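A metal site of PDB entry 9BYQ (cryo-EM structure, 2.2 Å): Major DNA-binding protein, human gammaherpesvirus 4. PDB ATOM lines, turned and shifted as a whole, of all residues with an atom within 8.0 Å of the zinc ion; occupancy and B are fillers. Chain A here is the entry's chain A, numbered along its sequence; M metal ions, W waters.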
ATOM      1  N   PRO A 106     -12.886   4.154  -0.172  1.00  0.00           N
ATOM      2  CA  PRO A 106     -11.675   4.788  -0.688  1.00  0.00           C
ATOM      3  C   PRO A 106     -11.658   6.333  -0.554  1.00  0.00           C
ATOM      4  O   PRO A 106     -12.686   6.964  -0.330  1.00  0.00           O
ATOM      5  CB  PRO A 106     -11.638   4.363  -2.165  1.00  0.00           C
ATOM      6  CG  PRO A 106     -13.111   4.295  -2.531  1.00  0.00           C
ATOM      7  CD  PRO A 106     -13.743   3.738  -1.273  1.00  0.00           C
ATOM      8  N   TYR A 443     -30.567   4.276  -5.204  1.00  0.00           N
ATOM      9  CA  TYR A 443     -29.477   5.203  -4.883  1.00  0.00           C
ATOM     10  C   TYR A 443     -28.108   4.564  -5.181  1.00  0.00           C
ATOM     11  O   TYR A 443     -27.304   5.138  -5.906  1.00  0.00           O
ATOM     12  CB  TYR A 443     -29.584   5.712  -3.450  1.00  0.00           C
ATOM     13  CG  TYR A 443     -28.492   6.712  -3.122  1.00  0.00           C
ATOM     14  CD1 TYR A 443     -28.643   8.065  -3.492  1.00  0.00           C
ATOM     15  CD2 TYR A 443     -27.294   6.276  -2.536  1.00  0.00           C
ATOM     16  CE1 TYR A 443     -27.610   8.974  -3.265  1.00  0.00           C
ATOM     17  CE2 TYR A 443     -26.246   7.183  -2.328  1.00  0.00           C
ATOM     18  CZ  TYR A 443     -26.397   8.536  -2.698  1.00  0.00           C
ATOM     19  OH  TYR A 443     -25.358   9.398  -2.539  1.00  0.00           O
ATOM     20  N   ALA A 447     -27.230   7.475  -8.350  1.00  0.00           N
ATOM     21  CA  ALA A 447     -26.312   8.587  -8.070  1.00  0.00           C
ATOM     22  C   ALA A 447     -24.998   8.221  -7.344  1.00  0.00           C
ATOM     23  O   ALA A 447     -23.989   8.893  -7.537  1.00  0.00           O
ATOM     24  CB  ALA A 447     -27.080   9.651  -7.278  1.00  0.00           C
ATOM     25  N   ALA A 448     -24.954   7.139  -6.550  1.00  0.00           N
ATOM     26  CA  ALA A 448     -23.702   6.705  -5.909  1.00  0.00           C
ATOM     27  C   ALA A 448     -22.629   6.200  -6.910  1.00  0.00           C
ATOM     28  O   ALA A 448     -21.447   6.255  -6.594  1.00  0.00           O
ATOM     29  CB  ALA A 448     -24.016   5.604  -4.903  1.00  0.00           C
ATOM     30  N   ALA A 449     -23.042   5.723  -8.082  1.00  0.00           N
ATOM     31  CA  ALA A 449     -22.177   5.175  -9.139  1.00  0.00           C
ATOM     32  C   ALA A 449     -21.703   6.250 -10.157  1.00  0.00           C
ATOM     33  O   ALA A 449     -21.048   5.914 -11.152  1.00  0.00           O
ATOM     34  CB  ALA A 449     -22.927   4.024  -9.808  1.00  0.00           C
ATOM     35  N   SER A 450     -22.032   7.525  -9.948  1.00  0.00           N
ATOM     36  CA  SER A 450     -21.644   8.633 -10.828  1.00  0.00           C
ATOM     37  C   SER A 450     -20.120   8.872 -10.835  1.00  0.00           C
ATOM     38  O   SER A 450     -19.507   8.915  -9.755  1.00  0.00           O
ATOM     39  CB  SER A 450     -22.364   9.905 -10.361  1.00  0.00           C
ATOM     40  OG  SER A 450     -21.951  11.024 -11.105  1.00  0.00           O
ATOM     41  N   MET A 452     -18.577  11.517 -10.982  1.00  0.00           N
ATOM     42  CA  MET A 452     -18.353  12.770 -10.264  1.00  0.00           C
ATOM     43  C   MET A 452     -17.970  12.622  -8.773  1.00  0.00           C
ATOM     44  O   MET A 452     -17.524  13.607  -8.185  1.00  0.00           O
ATOM     45  CB  MET A 452     -19.611  13.654 -10.385  1.00  0.00           C
ATOM     46  CG  MET A 452     -20.079  13.869 -11.823  1.00  0.00           C
ATOM     47  SD  MET A 452     -18.905  14.727 -12.900  1.00  0.00           S
ATOM     48  CE  MET A 452     -19.853  14.673 -14.444  1.00  0.00           C
ATOM     49  N   CYS A 453     -18.125  11.439  -8.147  1.00  0.00           N
ATOM     50  CA  CYS A 453     -17.732  11.209  -6.749  1.00  0.00           C
ATOM     51  C   CYS A 453     -16.219  11.414  -6.572  1.00  0.00           C
ATOM     52  O   CYS A 453     -15.402  10.712  -7.182  1.00  0.00           O
ATOM     53  CB  CYS A 453     -18.201   9.801  -6.306  1.00  0.00           C
ATOM     54  SG  CYS A 453     -17.942   9.490  -4.515  1.00  0.00           S
ATOM     55  N   SER A 454     -15.811  12.362  -5.728  1.00  0.00           N
ATOM     56  CA  SER A 454     -14.394  12.642  -5.412  1.00  0.00           C
ATOM     57  C   SER A 454     -13.739  11.618  -4.475  1.00  0.00           C
ATOM     58  O   SER A 454     -12.602  11.828  -4.052  1.00  0.00           O
ATOM     59  CB  SER A 454     -14.215  14.061  -4.863  1.00  0.00           C
ATOM     60  OG  SER A 454     -14.581  14.171  -3.493  1.00  0.00           O
ATOM     61  N   LEU A 455     -14.437  10.536  -4.109  1.00  0.00           N
ATOM     62  CA  LEU A 455     -13.936   9.506  -3.198  1.00  0.00           C
ATOM     63  C   LEU A 455     -13.747   8.152  -3.909  1.00  0.00           C
ATOM     64  O   LEU A 455     -12.627   7.628  -3.900  1.00  0.00           O
ATOM     65  CB  LEU A 455     -14.857   9.393  -1.961  1.00  0.00           C
ATOM     66  CG  LEU A 455     -15.108  10.697  -1.188  1.00  0.00           C
ATOM     67  CD1 LEU A 455     -15.932  10.421   0.062  1.00  0.00           C
ATOM     68  CD2 LEU A 455     -13.822  11.399  -0.752  1.00  0.00           C
ATOM     69  N   CYS A 456     -14.775   7.609  -4.558  1.00  0.00           N
ATOM     70  CA  CYS A 456     -14.762   6.299  -5.209  1.00  0.00           C
ATOM     71  C   CYS A 456     -14.744   6.348  -6.747  1.00  0.00           C
ATOM     72  O   CYS A 456     -14.573   5.308  -7.389  1.00  0.00           O
ATOM     73  CB  CYS A 456     -15.933   5.465  -4.674  1.00  0.00           C
ATOM     74  SG  CYS A 456     -17.529   6.209  -5.127  1.00  0.00           S
ATOM     75  N   GLU A 457     -14.898   7.521  -7.367  1.00  0.00           N
ATOM     76  CA  GLU A 457     -15.131   7.686  -8.810  1.00  0.00           C
ATOM     77  C   GLU A 457     -16.372   6.904  -9.309  1.00  0.00           C
ATOM     78  O   GLU A 457     -16.453   6.558 -10.485  1.00  0.00           O
ATOM     79  CB  GLU A 457     -13.875   7.366  -9.653  1.00  0.00           C
ATOM     80  CG  GLU A 457     -12.630   8.159  -9.254  1.00  0.00           C
ATOM     81  CD  GLU A 457     -11.446   7.825 -10.186  1.00  0.00           C
ATOM     82  OE1 GLU A 457     -11.241   6.630 -10.516  1.00  0.00           O
ATOM     83  OE2 GLU A 457     -10.699   8.747 -10.564  1.00  0.00           O
ATOM     84  N   GLY A 458     -17.300   6.543  -8.424  1.00  0.00           N
ATOM     85  CA  GLY A 458     -18.408   5.641  -8.709  1.00  0.00           C
ATOM     86  C   GLY A 458     -18.044   4.159  -8.705  1.00  0.00           C
ATOM     87  O   GLY A 458     -18.914   3.320  -8.934  1.00  0.00           O
ATOM     88  N   ARG A 459     -16.770   3.793  -8.467  1.00  0.00           N
ATOM     89  CA  ARG A 459     -16.251   2.407  -8.566  1.00  0.00           C
ATOM     90  C   ARG A 459     -16.337   1.587  -7.260  1.00  0.00           C
ATOM     91  O   ARG A 459     -15.926   0.433  -7.273  1.00  0.00           O
ATOM     92  CB  ARG A 459     -14.831   2.421  -9.168  1.00  0.00           C
ATOM     93  CG  ARG A 459     -14.748   3.105 -10.539  1.00  0.00           C
ATOM     94  CD  ARG A 459     -13.360   3.023 -11.207  1.00  0.00           C
ATOM     95  NE  ARG A 459     -12.338   3.838 -10.527  1.00  0.00           N
ATOM     96  CZ  ARG A 459     -11.457   3.449  -9.634  1.00  0.00           C
ATOM     97  NH1 ARG A 459     -10.656   4.327  -9.126  1.00  0.00           N
ATOM     98  NH2 ARG A 459     -11.347   2.213  -9.240  1.00  0.00           N
ATOM     99  N   ALA A 460     -16.884   2.128  -6.172  1.00  0.00           N
ATOM    100  CA  ALA A 460     -17.168   1.403  -4.921  1.00  0.00           C
ATOM    101  C   ALA A 460     -18.469   1.878  -4.218  1.00  0.00           C
ATOM    102  O   ALA A 460     -18.450   2.254  -3.046  1.00  0.00           O
ATOM    103  CB  ALA A 460     -15.939   1.492  -4.003  1.00  0.00           C
ATOM    104  N   PRO A 461     -19.628   1.904  -4.907  1.00  0.00           N
ATOM    105  CA  PRO A 461     -20.767   2.709  -4.516  1.00  0.00           C
ATOM    106  C   PRO A 461     -21.466   2.265  -3.219  1.00  0.00           C
ATOM    107  O   PRO A 461     -22.090   3.084  -2.549  1.00  0.00           O
ATOM    108  CB  PRO A 461     -21.716   2.670  -5.710  1.00  0.00           C
ATOM    109  CG  PRO A 461     -21.385   1.350  -6.388  1.00  0.00           C
ATOM    110  CD  PRO A 461     -19.883   1.239  -6.171  1.00  0.00           C
ATOM    111  N   ALA A 462     -21.391   0.982  -2.837  1.00  0.00           N
ATOM    112  CA  ALA A 462     -22.102   0.465  -1.672  1.00  0.00           C
ATOM    113  C   ALA A 462     -21.395   0.783  -0.329  1.00  0.00           C
ATOM    114  O   ALA A 462     -22.078   1.004   0.664  1.00  0.00           O
ATOM    115  CB  ALA A 462     -22.305  -1.037  -1.871  1.00  0.00           C
ATOM    116  N   VAL A 463     -20.064   0.863  -0.298  1.00  0.00           N
ATOM    117  CA  VAL A 463     -19.274   1.192   0.904  1.00  0.00           C
ATOM    118  C   VAL A 463     -18.809   2.658   0.997  1.00  0.00           C
ATOM    119  O   VAL A 463     -18.377   3.071   2.065  1.00  0.00           O
ATOM    120  CB  VAL A 463     -18.060   0.271   1.085  1.00  0.00           C
ATOM    121  CG1 VAL A 463     -18.512  -1.126   1.503  1.00  0.00           C
ATOM    122  CG2 VAL A 463     -17.150   0.187  -0.144  1.00  0.00           C
ATOM    123  N   CYS A 464     -18.921   3.455  -0.071  1.00  0.00           N
ATOM    124  CA  CYS A 464     -18.491   4.856  -0.101  1.00  0.00           C
ATOM    125  C   CYS A 464     -19.024   5.674   1.089  1.00  0.00           C
ATOM    126  O   CYS A 464     -20.188   5.543   1.488  1.00  0.00           O
ATOM    127  CB  CYS A 464     -18.869   5.467  -1.461  1.00  0.00           C
ATOM    128  SG  CYS A 464     -18.192   7.141  -1.660  1.00  0.00           S
ATOM    129  N   LEU A 465     -18.181   6.546   1.649  1.00  0.00           N
ATOM    130  CA  LEU A 465     -18.531   7.431   2.747  1.00  0.00           C
ATOM    131  C   LEU A 465     -19.736   8.326   2.406  1.00  0.00           C
ATOM    132  O   LEU A 465     -20.602   8.542   3.257  1.00  0.00           O
ATOM    133  CB  LEU A 465     -17.296   8.242   3.167  1.00  0.00           C
ATOM    134  CG  LEU A 465     -17.533   9.227   4.335  1.00  0.00           C
ATOM    135  CD1 LEU A 465     -17.907   8.529   5.634  1.00  0.00           C
ATOM    136  CD2 LEU A 465     -16.282  10.053   4.601  1.00  0.00           C
ATOM    137  N   ASN A 466     -19.868   8.793   1.165  1.00  0.00           N
ATOM    138  CA  ASN A 466     -21.033   9.567   0.719  1.00  0.00           C
ATOM    139  C   ASN A 466     -22.341   8.741   0.754  1.00  0.00           C
ATOM    140  O   ASN A 466     -23.403   9.304   1.008  1.00  0.00           O
ATOM    141  CB  ASN A 466     -20.766  10.131  -0.688  1.00  0.00           C
ATOM    142  CG  ASN A 466     -19.836  11.332  -0.696  1.00  0.00           C
ATOM    143  OD1 ASN A 466     -19.932  12.216   0.144  1.00  0.00           O
ATOM    144  ND2 ASN A 466     -18.972  11.445  -1.669  1.00  0.00           N
ATOM    145  N   THR A 467     -22.284   7.431   0.541  1.00  0.00           N
ATOM    146  CA  THR A 467     -23.450   6.535   0.672  1.00  0.00           C
ATOM    147  C   THR A 467     -23.860   6.359   2.136  1.00  0.00           C
ATOM    148  O   THR A 467     -25.042   6.488   2.447  1.00  0.00           O
ATOM    149  CB  THR A 467     -23.201   5.163   0.008  1.00  0.00           C
ATOM    150  OG1 THR A 467     -22.873   5.363  -1.341  1.00  0.00           O
ATOM    151  CG2 THR A 467     -24.412   4.245   0.040  1.00  0.00           C
HETATM  152 ZN    ZN M   1     -18.435   7.569  -4.010  1.00  0.00          ZN
HETATM  153  O   HOH W   1     -20.255   7.258  -4.240  1.00  0.00           O
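Three residues have an atom within 4 Å of the zinc ion: Cys 453, Cys 456 and Cys 464.
The zinc ion is bound by water W1 (1.9 Å), the side-chain sulfur of Cys 456 (2.0 Å), the side-chain sulfur of Cys 453 (2.0 Å) and the side-chain sulfur of Cys 464 (2.4 Å). The zinc ion has four donor atoms within binding distance.
The backbone NH of Gly 458 sits close to the side-chain sulfur of Cys 456, 3.3 Å away. The side-chain sulfur (SG) of Cys 453 lies close to the backbone NH (N) of Leu 455. The side-chain amide nitrogen (ND2) of Asn 466 lies close to the side-chain sulfur (SG) of Cys 453. SG of Cys 464 lies close to N of Asn 466 (3.7 Å).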
